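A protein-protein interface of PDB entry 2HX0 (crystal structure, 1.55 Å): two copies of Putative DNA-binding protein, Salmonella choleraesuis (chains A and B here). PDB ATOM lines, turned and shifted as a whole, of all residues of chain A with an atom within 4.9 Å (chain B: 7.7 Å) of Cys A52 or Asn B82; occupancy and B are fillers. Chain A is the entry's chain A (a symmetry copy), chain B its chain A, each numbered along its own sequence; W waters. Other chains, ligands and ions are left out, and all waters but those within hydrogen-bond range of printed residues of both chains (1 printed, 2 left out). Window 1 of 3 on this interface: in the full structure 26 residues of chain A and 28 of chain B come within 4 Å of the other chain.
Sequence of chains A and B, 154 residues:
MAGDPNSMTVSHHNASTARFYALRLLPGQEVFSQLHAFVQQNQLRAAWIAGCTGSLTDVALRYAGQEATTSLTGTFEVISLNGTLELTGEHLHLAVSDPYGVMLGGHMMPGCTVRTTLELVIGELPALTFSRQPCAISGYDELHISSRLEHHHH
Among the printed residues, merely in contact across the chains: Gly A51 with Trp B48, Cys A52 with Asn B82, Thr A53 with His B91, Gly A54 with His B93, Ile A79 with Ser B80, Ile A79 with Ala B95, Ile A79 with Gly B106 and Ser A80 with Asn B82.
Cys A52 touches just one residue of chain B: Asn B82. Ile B49 touches none of the printed residues of chain A. Of chain A, only Cys A52 (3.5 Å), Ile A79 (3.3 Å) and Ser A80 (3.96 Å) come within 4 Å of Asn B82. Of the printed residues of chain A, Thr B84 touches Glu A119 (2.7 Å). Leu B94 touches none of the printed residues of chain A. Of the printed residues of chain A, Ala B95 touches Ile A79 (3.4 Å). The nearest residue of chain B that does not touch Cys A52 is Gly B83 (4.5 Å). The nearest residue of chain A that does not touch Asn B82 is Thr A53 (4.4 Å). The nearest printed residue of chain A that does not touch Ser B80 is Ser A80 (4.6 Å).
Water W1 lies within hydrogen-bond range of O of Ile A79 (2.7 Å), OG of Ser B80 (2.9 Å), ND2 of Asn B82 (3.0 Å) and O of His B93 (3.1 Å).
Hydrophobic or aromatic side chains of chain B that line the printed part of chain A: Trp B48, His B91, His B93 and Ala B95. Printed residues of chain A that touch a printed residue of chain B: Ala A50, Gly A51, Cys A52, Thr A53, Gly A54, Val A78, Ile A79, Ser A80 and Glu A119. Hydrophobic or aromatic side chains of chain A within 4 Å of the printed part of chain B: Ala A50 and Ile A79. Among the printed residues, 14 pairs touch across the chains. Among the printed residues, no Asp or Glu carboxylate lies within 4 Å of a Lys or Arg side-chain nitrogen of the other chain.
The backbone NH (N) of Ile B79 lies within hydrogen-bond range of the backbone carbonyl oxygen (O) of Ala B95 (2.9 Å). N of Glu A119 sits at hydrogen-bond distance from O of Thr A53 (2.7 Å). The backbone NH (N) of His B91 is in hydrogen-bond range of the backbone carbonyl oxygen (O) of Thr B84. The backbone NH of His B93 sits at hydrogen-bond distance from the backbone carbonyl oxygen of Asn B82 (2.8 Å). The side-chain sulfur (SG) of Cys A52 lies close to the backbone carbonyl oxygen (O) of Glu A119 (3.7 Å). The backbone carbonyl oxygen (O) of Ser B80 sits at hydrogen-bond distance from the backbone NH (N) of Ala B95 (2.9 Å).
Ile A79 touches Ser B80, but with the chains exchanged Ser A80 does not touch Ile B79 (7.2 Å). Positions printed for both chains: 49, 50, 51, 52, 78, 79, 80 and 81. Of the 14 pairs that touch across the chains among the printed residues, none has its exchanged pair printed and touching as well.
ND1 of His B93 lies within hydrogen-bond range of OG1 of Thr A53 (3.2 Å). ND1 of His B93 lies within hydrogen-bond range of O of Val A78, at 2.7 Å. The indole nitrogen (NE1) of Trp B48 sits at hydrogen-bond distance from the backbone carbonyl oxygen (O) of Ala A50 (3.0 Å). OE2 of Glu A119 sits at hydrogen-bond distance from ND1 of His B91, 2.7 Å away. The side-chain hydroxyl (OG1) of Thr B84 lies within hydrogen-bond range of the side-chain carboxylate (OE1) of Glu A119 (2.7 Å). The side-chain amide nitrogen (ND2) of Asn B82 lies within hydrogen-bond range of the backbone carbonyl oxygen (O) of Ile A79, 3.3 Å away.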
ATOM      1  N   ILE A  49      27.907 -11.315   7.273  1.00  0.00           N
ATOM      2  CA  ILE A  49      27.886 -10.755   5.927  1.00  0.00           C
ATOM      3  C   ILE A  49      26.721  -9.778   5.862  1.00  0.00           C
ATOM      4  O   ILE A  49      25.559 -10.181   5.924  1.00  0.00           O
ATOM      5  CB  ILE A  49      27.675 -11.844   4.864  1.00  0.00           C
ATOM      6  CG1 ILE A  49      28.672 -12.987   5.073  1.00  0.00           C
ATOM      7  CG2 ILE A  49      27.847 -11.232   3.479  1.00  0.00           C
ATOM      8  CD1 ILE A  49      30.187 -12.647   4.989  1.00  0.00           C
ATOM      9  N   ALA A  50      27.039  -8.491   5.748  1.00  0.00           N
ATOM     10  CA  ALA A  50      26.011  -7.457   5.701  1.00  0.00           C
ATOM     11  C   ALA A  50      25.517  -7.170   4.290  1.00  0.00           C
ATOM     12  O   ALA A  50      24.446  -6.596   4.109  1.00  0.00           O
ATOM     13  CB  ALA A  50      26.535  -6.167   6.346  1.00  0.00           C
ATOM     14  N   GLY A  51      26.298  -7.563   3.293  1.00  0.00           N
ATOM     15  CA  GLY A  51      25.905  -7.337   1.913  1.00  0.00           C
ATOM     16  C   GLY A  51      26.827  -8.097   0.985  1.00  0.00           C
ATOM     17  O   GLY A  51      28.020  -8.209   1.258  1.00  0.00           O
ATOM     18  N   CYS A  52      26.287  -8.632  -0.105  1.00  0.00           N
ATOM     19  CA  CYS A  52      27.116  -9.377  -1.045  1.00  0.00           C
ATOM     20  C   CYS A  52      26.487  -9.524  -2.418  1.00  0.00           C
ATOM     21  O   CYS A  52      25.292  -9.803  -2.548  1.00  0.00           O
ATOM     22  CB  CYS A  52      27.428 -10.774  -0.487  1.00  0.00           C
ATOM     23  SG  CYS A  52      28.466 -11.815  -1.564  1.00  0.00           S
ATOM     24  N   THR A  53      27.302  -9.319  -3.444  1.00  0.00           N
ATOM     25  CA  THR A  53      26.846  -9.468  -4.816  1.00  0.00           C
ATOM     26  C   THR A  53      28.041  -9.921  -5.632  1.00  0.00           C
ATOM     27  O   THR A  53      29.178  -9.601  -5.301  1.00  0.00           O
ATOM     28  CB  THR A  53      26.302  -8.150  -5.387  1.00  0.00           C
ATOM     29  OG1 THR A  53      25.765  -8.391  -6.693  1.00  0.00           O
ATOM     30  CG2 THR A  53      27.398  -7.106  -5.484  1.00  0.00           C
ATOM     31  N   GLY A  54      27.790 -10.677  -6.693  1.00  0.00           N
ATOM     32  CA  GLY A  54      28.890 -11.146  -7.509  1.00  0.00           C
ATOM     33  C   GLY A  54      28.520 -12.315  -8.390  1.00  0.00           C
ATOM     34  O   GLY A  54      27.345 -12.584  -8.621  1.00  0.00           O
ATOM     35  N   VAL A  78      25.633 -14.598  -7.739  1.00  0.00           N
ATOM     36  CA  VAL A  78      25.423 -14.749  -6.306  1.00  0.00           C
ATOM     37  C   VAL A  78      24.248 -13.849  -5.957  1.00  0.00           C
ATOM     38  O   VAL A  78      24.318 -12.627  -6.113  1.00  0.00           O
ATOM     39  CB  VAL A  78      26.655 -14.318  -5.500  1.00  0.00           C
ATOM     40  CG1 VAL A  78      26.318 -14.304  -4.017  1.00  0.00           C
ATOM     41  CG2 VAL A  78      27.802 -15.275  -5.766  1.00  0.00           C
ATOM     42  N   ILE A  79      23.160 -14.452  -5.493  1.00  0.00           N
ATOM     43  CA  ILE A  79      21.967 -13.690  -5.146  1.00  0.00           C
ATOM     44  C   ILE A  79      22.022 -13.267  -3.691  1.00  0.00           C
ATOM     45  O   ILE A  79      21.631 -12.152  -3.337  1.00  0.00           O
ATOM     46  CB  ILE A  79      20.696 -14.515  -5.420  1.00  0.00           C
ATOM     47  CG1 ILE A  79      20.571 -14.769  -6.927  1.00  0.00           C
ATOM     48  CG2 ILE A  79      19.462 -13.783  -4.906  1.00  0.00           C
ATOM     49  CD1 ILE A  79      19.262 -15.200  -7.492  1.00  0.00           C
ATOM     50  N   SER A  80      22.512 -14.161  -2.847  1.00  0.00           N
ATOM     51  CA  SER A  80      22.651 -13.844  -1.438  1.00  0.00           C
ATOM     52  C   SER A  80      23.658 -14.762  -0.775  1.00  0.00           C
ATOM     53  O   SER A  80      23.758 -15.946  -1.097  1.00  0.00           O
ATOM     54  CB  SER A  80      21.307 -13.942  -0.715  1.00  0.00           C
ATOM     55  OG  SER A  80      20.817 -15.265  -0.710  1.00  0.00           O
ATOM     56  N   LEU A  81      24.425 -14.183   0.134  1.00  0.00           N
ATOM     57  CA  LEU A  81      25.421 -14.903   0.904  1.00  0.00           C
ATOM     58  C   LEU A  81      25.189 -14.350   2.295  1.00  0.00           C
ATOM     59  O   LEU A  81      25.448 -13.177   2.556  1.00  0.00           O
ATOM     60  CB  LEU A  81      26.834 -14.566   0.424  1.00  0.00           C
ATOM     61  CG  LEU A  81      27.939 -15.117   1.328  1.00  0.00           C
ATOM     62  CD1 LEU A  81      27.871 -16.630   1.347  1.00  0.00           C
ATOM     63  CD2 LEU A  81      29.293 -14.640   0.826  1.00  0.00           C
ATOM     64  N   LEU A 118      33.325 -10.576  -6.599  1.00  0.00           N
ATOM     65  CA  LEU A 118      32.484 -10.846  -5.439  1.00  0.00           C
ATOM     66  C   LEU A 118      32.666  -9.620  -4.561  1.00  0.00           C
ATOM     67  O   LEU A 118      33.747  -9.381  -4.028  1.00  0.00           O
ATOM     68  CB  LEU A 118      32.888 -12.111  -4.679  1.00  0.00           C
ATOM     69  CG  LEU A 118      31.759 -12.470  -3.697  1.00  0.00           C
ATOM     70  CD1 LEU A 118      30.545 -12.961  -4.487  1.00  0.00           C
ATOM     71  CD2 LEU A 118      32.214 -13.537  -2.716  1.00  0.00           C
ATOM     72  N   GLU A 119      31.609  -8.820  -4.447  1.00  0.00           N
ATOM     73  CA  GLU A 119      31.639  -7.598  -3.652  1.00  0.00           C
ATOM     74  C   GLU A 119      31.012  -7.901  -2.308  1.00  0.00           C
ATOM     75  O   GLU A 119      29.913  -8.438  -2.243  1.00  0.00           O
ATOM     76  CB  GLU A 119      30.859  -6.501  -4.368  1.00  0.00           C
ATOM     77  CG  GLU A 119      31.519  -6.043  -5.666  1.00  0.00           C
ATOM     78  CD  GLU A 119      30.634  -5.127  -6.492  1.00  0.00           C
ATOM     79  OE1 GLU A 119      29.879  -4.326  -5.901  1.00  0.00           O
ATOM     80  OE2 GLU A 119      30.706  -5.196  -7.739  1.00  0.00           O
ATOM     81  N   LEU A 120      31.713  -7.545  -1.239  1.00  0.00           N
ATOM     82  CA  LEU A 120      31.230  -7.832   0.099  1.00  0.00           C
ATOM     83  C   LEU A 120      31.317  -6.676   1.071  1.00  0.00           C
ATOM     84  O   LEU A 120      32.254  -5.885   1.033  1.00  0.00           O
ATOM     85  CB  LEU A 120      32.048  -8.977   0.707  1.00  0.00           C
ATOM     86  CG  LEU A 120      32.008 -10.383   0.119  1.00  0.00           C
ATOM     87  CD1 LEU A 120      33.381 -11.022   0.242  1.00  0.00           C
ATOM     88  CD2 LEU A 120      30.960 -11.206   0.855  1.00  0.00           C
ATOM     89  N   TRP B  48      25.311   0.441   0.322  1.00  0.00           N
ATOM     90  CA  TRP B  48      24.924  -0.931   0.017  1.00  0.00           C
ATOM     91  C   TRP B  48      23.525  -1.147   0.572  1.00  0.00           C
ATOM     92  O   TRP B  48      23.080  -0.407   1.450  1.00  0.00           O
ATOM     93  CB  TRP B  48      25.933  -1.925   0.630  1.00  0.00           C
ATOM     94  CG  TRP B  48      25.664  -2.387   2.046  1.00  0.00           C
ATOM     95  CD1 TRP B  48      25.041  -3.541   2.429  1.00  0.00           C
ATOM     96  CD2 TRP B  48      26.062  -1.728   3.253  1.00  0.00           C
ATOM     97  NE1 TRP B  48      25.029  -3.643   3.800  1.00  0.00           N
ATOM     98  CE2 TRP B  48      25.649  -2.542   4.331  1.00  0.00           C
ATOM     99  CE3 TRP B  48      26.728  -0.526   3.529  1.00  0.00           C
ATOM    100  CZ2 TRP B  48      25.884  -2.195   5.667  1.00  0.00           C
ATOM    101  CZ3 TRP B  48      26.960  -0.179   4.856  1.00  0.00           C
ATOM    102  CH2 TRP B  48      26.537  -1.014   5.910  1.00  0.00           C
ATOM    103  N   ILE B  49      22.816  -2.132   0.037  1.00  0.00           N
ATOM    104  CA  ILE B  49      21.470  -2.416   0.520  1.00  0.00           C
ATOM    105  C   ILE B  49      21.608  -3.304   1.749  1.00  0.00           C
ATOM    106  O   ILE B  49      22.028  -4.458   1.647  1.00  0.00           O
ATOM    107  CB  ILE B  49      20.635  -3.162  -0.533  1.00  0.00           C
ATOM    108  CG1 ILE B  49      20.700  -2.426  -1.875  1.00  0.00           C
ATOM    109  CG2 ILE B  49      19.194  -3.267  -0.049  1.00  0.00           C
ATOM    110  CD1 ILE B  49      20.172  -0.964  -1.921  1.00  0.00           C
ATOM    111  N   ALA B  50      21.266  -2.756   2.911  1.00  0.00           N
ATOM    112  CA  ALA B  50      21.378  -3.497   4.163  1.00  0.00           C
ATOM    113  C   ALA B  50      20.128  -4.302   4.494  1.00  0.00           C
ATOM    114  O   ALA B  50      20.178  -5.225   5.304  1.00  0.00           O
ATOM    115  CB  ALA B  50      21.705  -2.538   5.314  1.00  0.00           C
ATOM    116  N   GLY B  51      19.010  -3.950   3.874  1.00  0.00           N
ATOM    117  CA  GLY B  51      17.771  -4.665   4.123  1.00  0.00           C
ATOM    118  C   GLY B  51      16.723  -4.243   3.117  1.00  0.00           C
ATOM    119  O   GLY B  51      16.676  -3.079   2.729  1.00  0.00           O
ATOM    120  N   CYS B  52      15.889  -5.180   2.679  1.00  0.00           N
ATOM    121  CA  CYS B  52      14.852  -4.844   1.709  1.00  0.00           C
ATOM    122  C   CYS B  52      13.726  -5.860   1.656  1.00  0.00           C
ATOM    123  O   CYS B  52      13.956  -7.072   1.672  1.00  0.00           O
ATOM    124  CB  CYS B  52      15.462  -4.702   0.307  1.00  0.00           C
ATOM    125  SG  CYS B  52      14.274  -4.278  -1.007  1.00  0.00           S
ATOM    126  N   VAL B  78       9.455  -9.319  -3.303  1.00  0.00           N
ATOM    127  CA  VAL B  78      10.898  -9.133  -3.329  1.00  0.00           C
ATOM    128  C   VAL B  78      11.446  -9.927  -2.152  1.00  0.00           C
ATOM    129  O   VAL B  78      11.136  -9.636  -0.994  1.00  0.00           O
ATOM    130  CB  VAL B  78      11.288  -7.657  -3.175  1.00  0.00           C
ATOM    131  CG1 VAL B  78      12.795  -7.540  -3.007  1.00  0.00           C
ATOM    132  CG2 VAL B  78      10.835  -6.878  -4.396  1.00  0.00           C
ATOM    133  N   ILE B  79      12.251 -10.940  -2.447  1.00  0.00           N
ATOM    134  CA  ILE B  79      12.816 -11.781  -1.400  1.00  0.00           C
ATOM    135  C   ILE B  79      14.144 -11.216  -0.934  1.00  0.00           C
ATOM    136  O   ILE B  79      14.459 -11.230   0.258  1.00  0.00           O
ATOM    137  CB  ILE B  79      12.992 -13.227  -1.901  1.00  0.00           C
ATOM    138  CG1 ILE B  79      11.614 -13.835  -2.187  1.00  0.00           C
ATOM    139  CG2 ILE B  79      13.732 -14.066  -0.864  1.00  0.00           C
ATOM    140  CD1 ILE B  79      11.477 -15.314  -2.311  1.00  0.00           C
ATOM    141  N   SER B  80      14.923 -10.714  -1.880  1.00  0.00           N
ATOM    142  CA  SER B  80      16.195 -10.106  -1.540  1.00  0.00           C
ATOM    143  C   SER B  80      16.664  -9.180  -2.644  1.00  0.00           C
ATOM    144  O   SER B  80      16.466  -9.442  -3.831  1.00  0.00           O
ATOM    145  CB  SER B  80      17.260 -11.171  -1.270  1.00  0.00           C
ATOM    146  OG  SER B  80      17.549 -11.919  -2.431  1.00  0.00           O
ATOM    147  N   LEU B  81      17.260  -8.074  -2.227  1.00  0.00           N
ATOM    148  CA  LEU B  81      17.811  -7.083  -3.133  1.00  0.00           C
ATOM    149  C   LEU B  81      19.139  -6.775  -2.473  1.00  0.00           C
ATOM    150  O   LEU B  81      19.183  -6.199  -1.388  1.00  0.00           O
ATOM    151  CB  LEU B  81      16.932  -5.832  -3.175  1.00  0.00           C
ATOM    152  CG  LEU B  81      17.562  -4.664  -3.937  1.00  0.00           C
ATOM    153  CD1 LEU B  81      17.773  -5.057  -5.384  1.00  0.00           C
ATOM    154  CD2 LEU B  81      16.663  -3.442  -3.831  1.00  0.00           C
ATOM    155  N   ASN B  82      20.219  -7.192  -3.116  1.00  0.00           N
ATOM    156  CA  ASN B  82      21.542  -6.998  -2.554  1.00  0.00           C
ATOM    157  C   ASN B  82      22.492  -6.306  -3.497  1.00  0.00           C
ATOM    158  O   ASN B  82      22.333  -6.354  -4.717  1.00  0.00           O
ATOM    159  CB  ASN B  82      22.135  -8.348  -2.149  1.00  0.00           C
ATOM    160  CG  ASN B  82      21.515  -8.901  -0.884  1.00  0.00           C
ATOM    161  OD1 ASN B  82      21.661  -8.322   0.194  1.00  0.00           O
ATOM    162  ND2 ASN B  82      20.816 -10.022  -1.007  1.00  0.00           N
ATOM    163  N   GLY B  83      23.491  -5.654  -2.926  1.00  0.00           N
ATOM    164  CA  GLY B  83      24.453  -4.986  -3.765  1.00  0.00           C
ATOM    165  C   GLY B  83      24.893  -3.642  -3.250  1.00  0.00           C
ATOM    166  O   GLY B  83      24.430  -3.157  -2.215  1.00  0.00           O
ATOM    167  N   THR B  84      25.794  -3.039  -4.010  1.00  0.00           N
ATOM    168  CA  THR B  84      26.373  -1.754  -3.684  1.00  0.00           C
ATOM    169  C   THR B  84      25.862  -0.687  -4.630  1.00  0.00           C
ATOM    170  O   THR B  84      25.378  -0.987  -5.717  1.00  0.00           O
ATOM    171  CB  THR B  84      27.900  -1.828  -3.821  1.00  0.00           C
ATOM    172  OG1 THR B  84      28.231  -2.341  -5.125  1.00  0.00           O
ATOM    173  CG2 THR B  84      28.484  -2.749  -2.761  1.00  0.00           C
ATOM    174  N   LEU B  85      25.949   0.564  -4.206  1.00  0.00           N
ATOM    175  CA  LEU B  85      25.532   1.658  -5.062  1.00  0.00           C
ATOM    176  C   LEU B  85      26.203   2.930  -4.591  1.00  0.00           C
ATOM    177  O   LEU B  85      26.556   3.066  -3.419  1.00  0.00           O
ATOM    178  CB  LEU B  85      24.003   1.812  -5.077  1.00  0.00           C
ATOM    179  CG  LEU B  85      23.215   2.197  -3.827  1.00  0.00           C
ATOM    180  CD1 LEU B  85      21.762   2.414  -4.216  1.00  0.00           C
ATOM    181  CD2 LEU B  85      23.326   1.116  -2.764  1.00  0.00           C
ATOM    182  N   HIS B  91      25.754  -2.084  -8.432  1.00  0.00           N
ATOM    183  CA  HIS B  91      25.805  -3.495  -8.796  1.00  0.00           C
ATOM    184  C   HIS B  91      24.794  -4.148  -7.871  1.00  0.00           C
ATOM    185  O   HIS B  91      25.096  -4.430  -6.712  1.00  0.00           O
ATOM    186  CB  HIS B  91      27.205  -4.079  -8.568  1.00  0.00           C
ATOM    187  CG  HIS B  91      27.379  -5.459  -9.127  1.00  0.00           C
ATOM    188  ND1 HIS B  91      28.577  -6.140  -9.078  1.00  0.00           N
ATOM    189  CD2 HIS B  91      26.503  -6.285  -9.748  1.00  0.00           C
ATOM    190  CE1 HIS B  91      28.433  -7.324  -9.648  1.00  0.00           C
ATOM    191  NE2 HIS B  91      27.184  -7.436 -10.064  1.00  0.00           N
ATOM    192  N   LEU B  92      23.590  -4.376  -8.389  1.00  0.00           N
ATOM    193  CA  LEU B  92      22.510  -4.953  -7.593  1.00  0.00           C
ATOM    194  C   LEU B  92      21.931  -6.231  -8.174  1.00  0.00           C
ATOM    195  O   LEU B  92      21.728  -6.334  -9.380  1.00  0.00           O
ATOM    196  CB  LEU B  92      21.383  -3.924  -7.443  1.00  0.00           C
ATOM    197  CG  LEU B  92      21.804  -2.573  -6.857  1.00  0.00           C
ATOM    198  CD1 LEU B  92      20.721  -1.532  -7.081  1.00  0.00           C
ATOM    199  CD2 LEU B  92      22.096  -2.746  -5.382  1.00  0.00           C
ATOM    200  N   HIS B  93      21.670  -7.200  -7.305  1.00  0.00           N
ATOM    201  CA  HIS B  93      21.071  -8.466  -7.710  1.00  0.00           C
ATOM    202  C   HIS B  93      19.726  -8.581  -7.014  1.00  0.00           C
ATOM    203  O   HIS B  93      19.571  -8.158  -5.869  1.00  0.00           O
ATOM    204  CB  HIS B  93      21.979  -9.639  -7.340  1.00  0.00           C
ATOM    205  CG  HIS B  93      23.170  -9.772  -8.237  1.00  0.00           C
ATOM    206  ND1 HIS B  93      24.112 -10.766  -8.087  1.00  0.00           N
ATOM    207  CD2 HIS B  93      23.561  -9.044  -9.311  1.00  0.00           C
ATOM    208  CE1 HIS B  93      25.030 -10.648  -9.030  1.00  0.00           C
ATOM    209  NE2 HIS B  93      24.720  -9.611  -9.786  1.00  0.00           N
ATOM    210  N   LEU B  94      18.755  -9.155  -7.713  1.00  0.00           N
ATOM    211  CA  LEU B  94      17.403  -9.279  -7.187  1.00  0.00           C
ATOM    212  C   LEU B  94      16.853 -10.692  -7.259  1.00  0.00           C
ATOM    213  O   LEU B  94      17.108 -11.417  -8.220  1.00  0.00           O
ATOM    214  CB  LEU B  94      16.480  -8.343  -7.974  1.00  0.00           C
ATOM    215  CG  LEU B  94      14.959  -8.433  -7.785  1.00  0.00           C
ATOM    216  CD1 LEU B  94      14.558  -7.919  -6.412  1.00  0.00           C
ATOM    217  CD2 LEU B  94      14.273  -7.612  -8.871  1.00  0.00           C
ATOM    218  N   ALA B  95      16.100 -11.074  -6.229  1.00  0.00           N
ATOM    219  CA  ALA B  95      15.448 -12.381  -6.177  1.00  0.00           C
ATOM    220  C   ALA B  95      13.979 -12.111  -5.853  1.00  0.00           C
ATOM    221  O   ALA B  95      13.669 -11.423  -4.879  1.00  0.00           O
ATOM    222  CB  ALA B  95      16.077 -13.258  -5.091  1.00  0.00           C
ATOM    223  N   GLY B 106      18.622 -12.738 -10.560  1.00  0.00           N
ATOM    224  CA  GLY B 106      19.556 -12.268 -11.562  1.00  0.00           C
ATOM    225  C   GLY B 106      20.063 -10.874 -11.262  1.00  0.00           C
ATOM    226  O   GLY B 106      19.827 -10.331 -10.182  1.00  0.00           O
ATOM    227  N   MET B 108      19.885  -7.131 -11.386  1.00  0.00           N
ATOM    228  CA  MET B 108      18.765  -6.213 -11.516  1.00  0.00           C
ATOM    229  C   MET B 108      19.021  -5.143 -12.569  1.00  0.00           C
ATOM    230  O   MET B 108      20.098  -4.554 -12.624  1.00  0.00           O
ATOM    231  CB  MET B 108      18.453  -5.552 -10.172  1.00  0.00           C
ATOM    232  CG  MET B 108      17.205  -4.695 -10.200  1.00  0.00           C
ATOM    233  SD  MET B 108      16.663  -4.168  -8.428  1.00  0.00           S
ATOM    234  CE  MET B 108      17.431  -2.401  -8.379  1.00  0.00           C
HETATM  235  O   HOH W   1      19.657 -10.401  -3.794  1.00  0.00           O
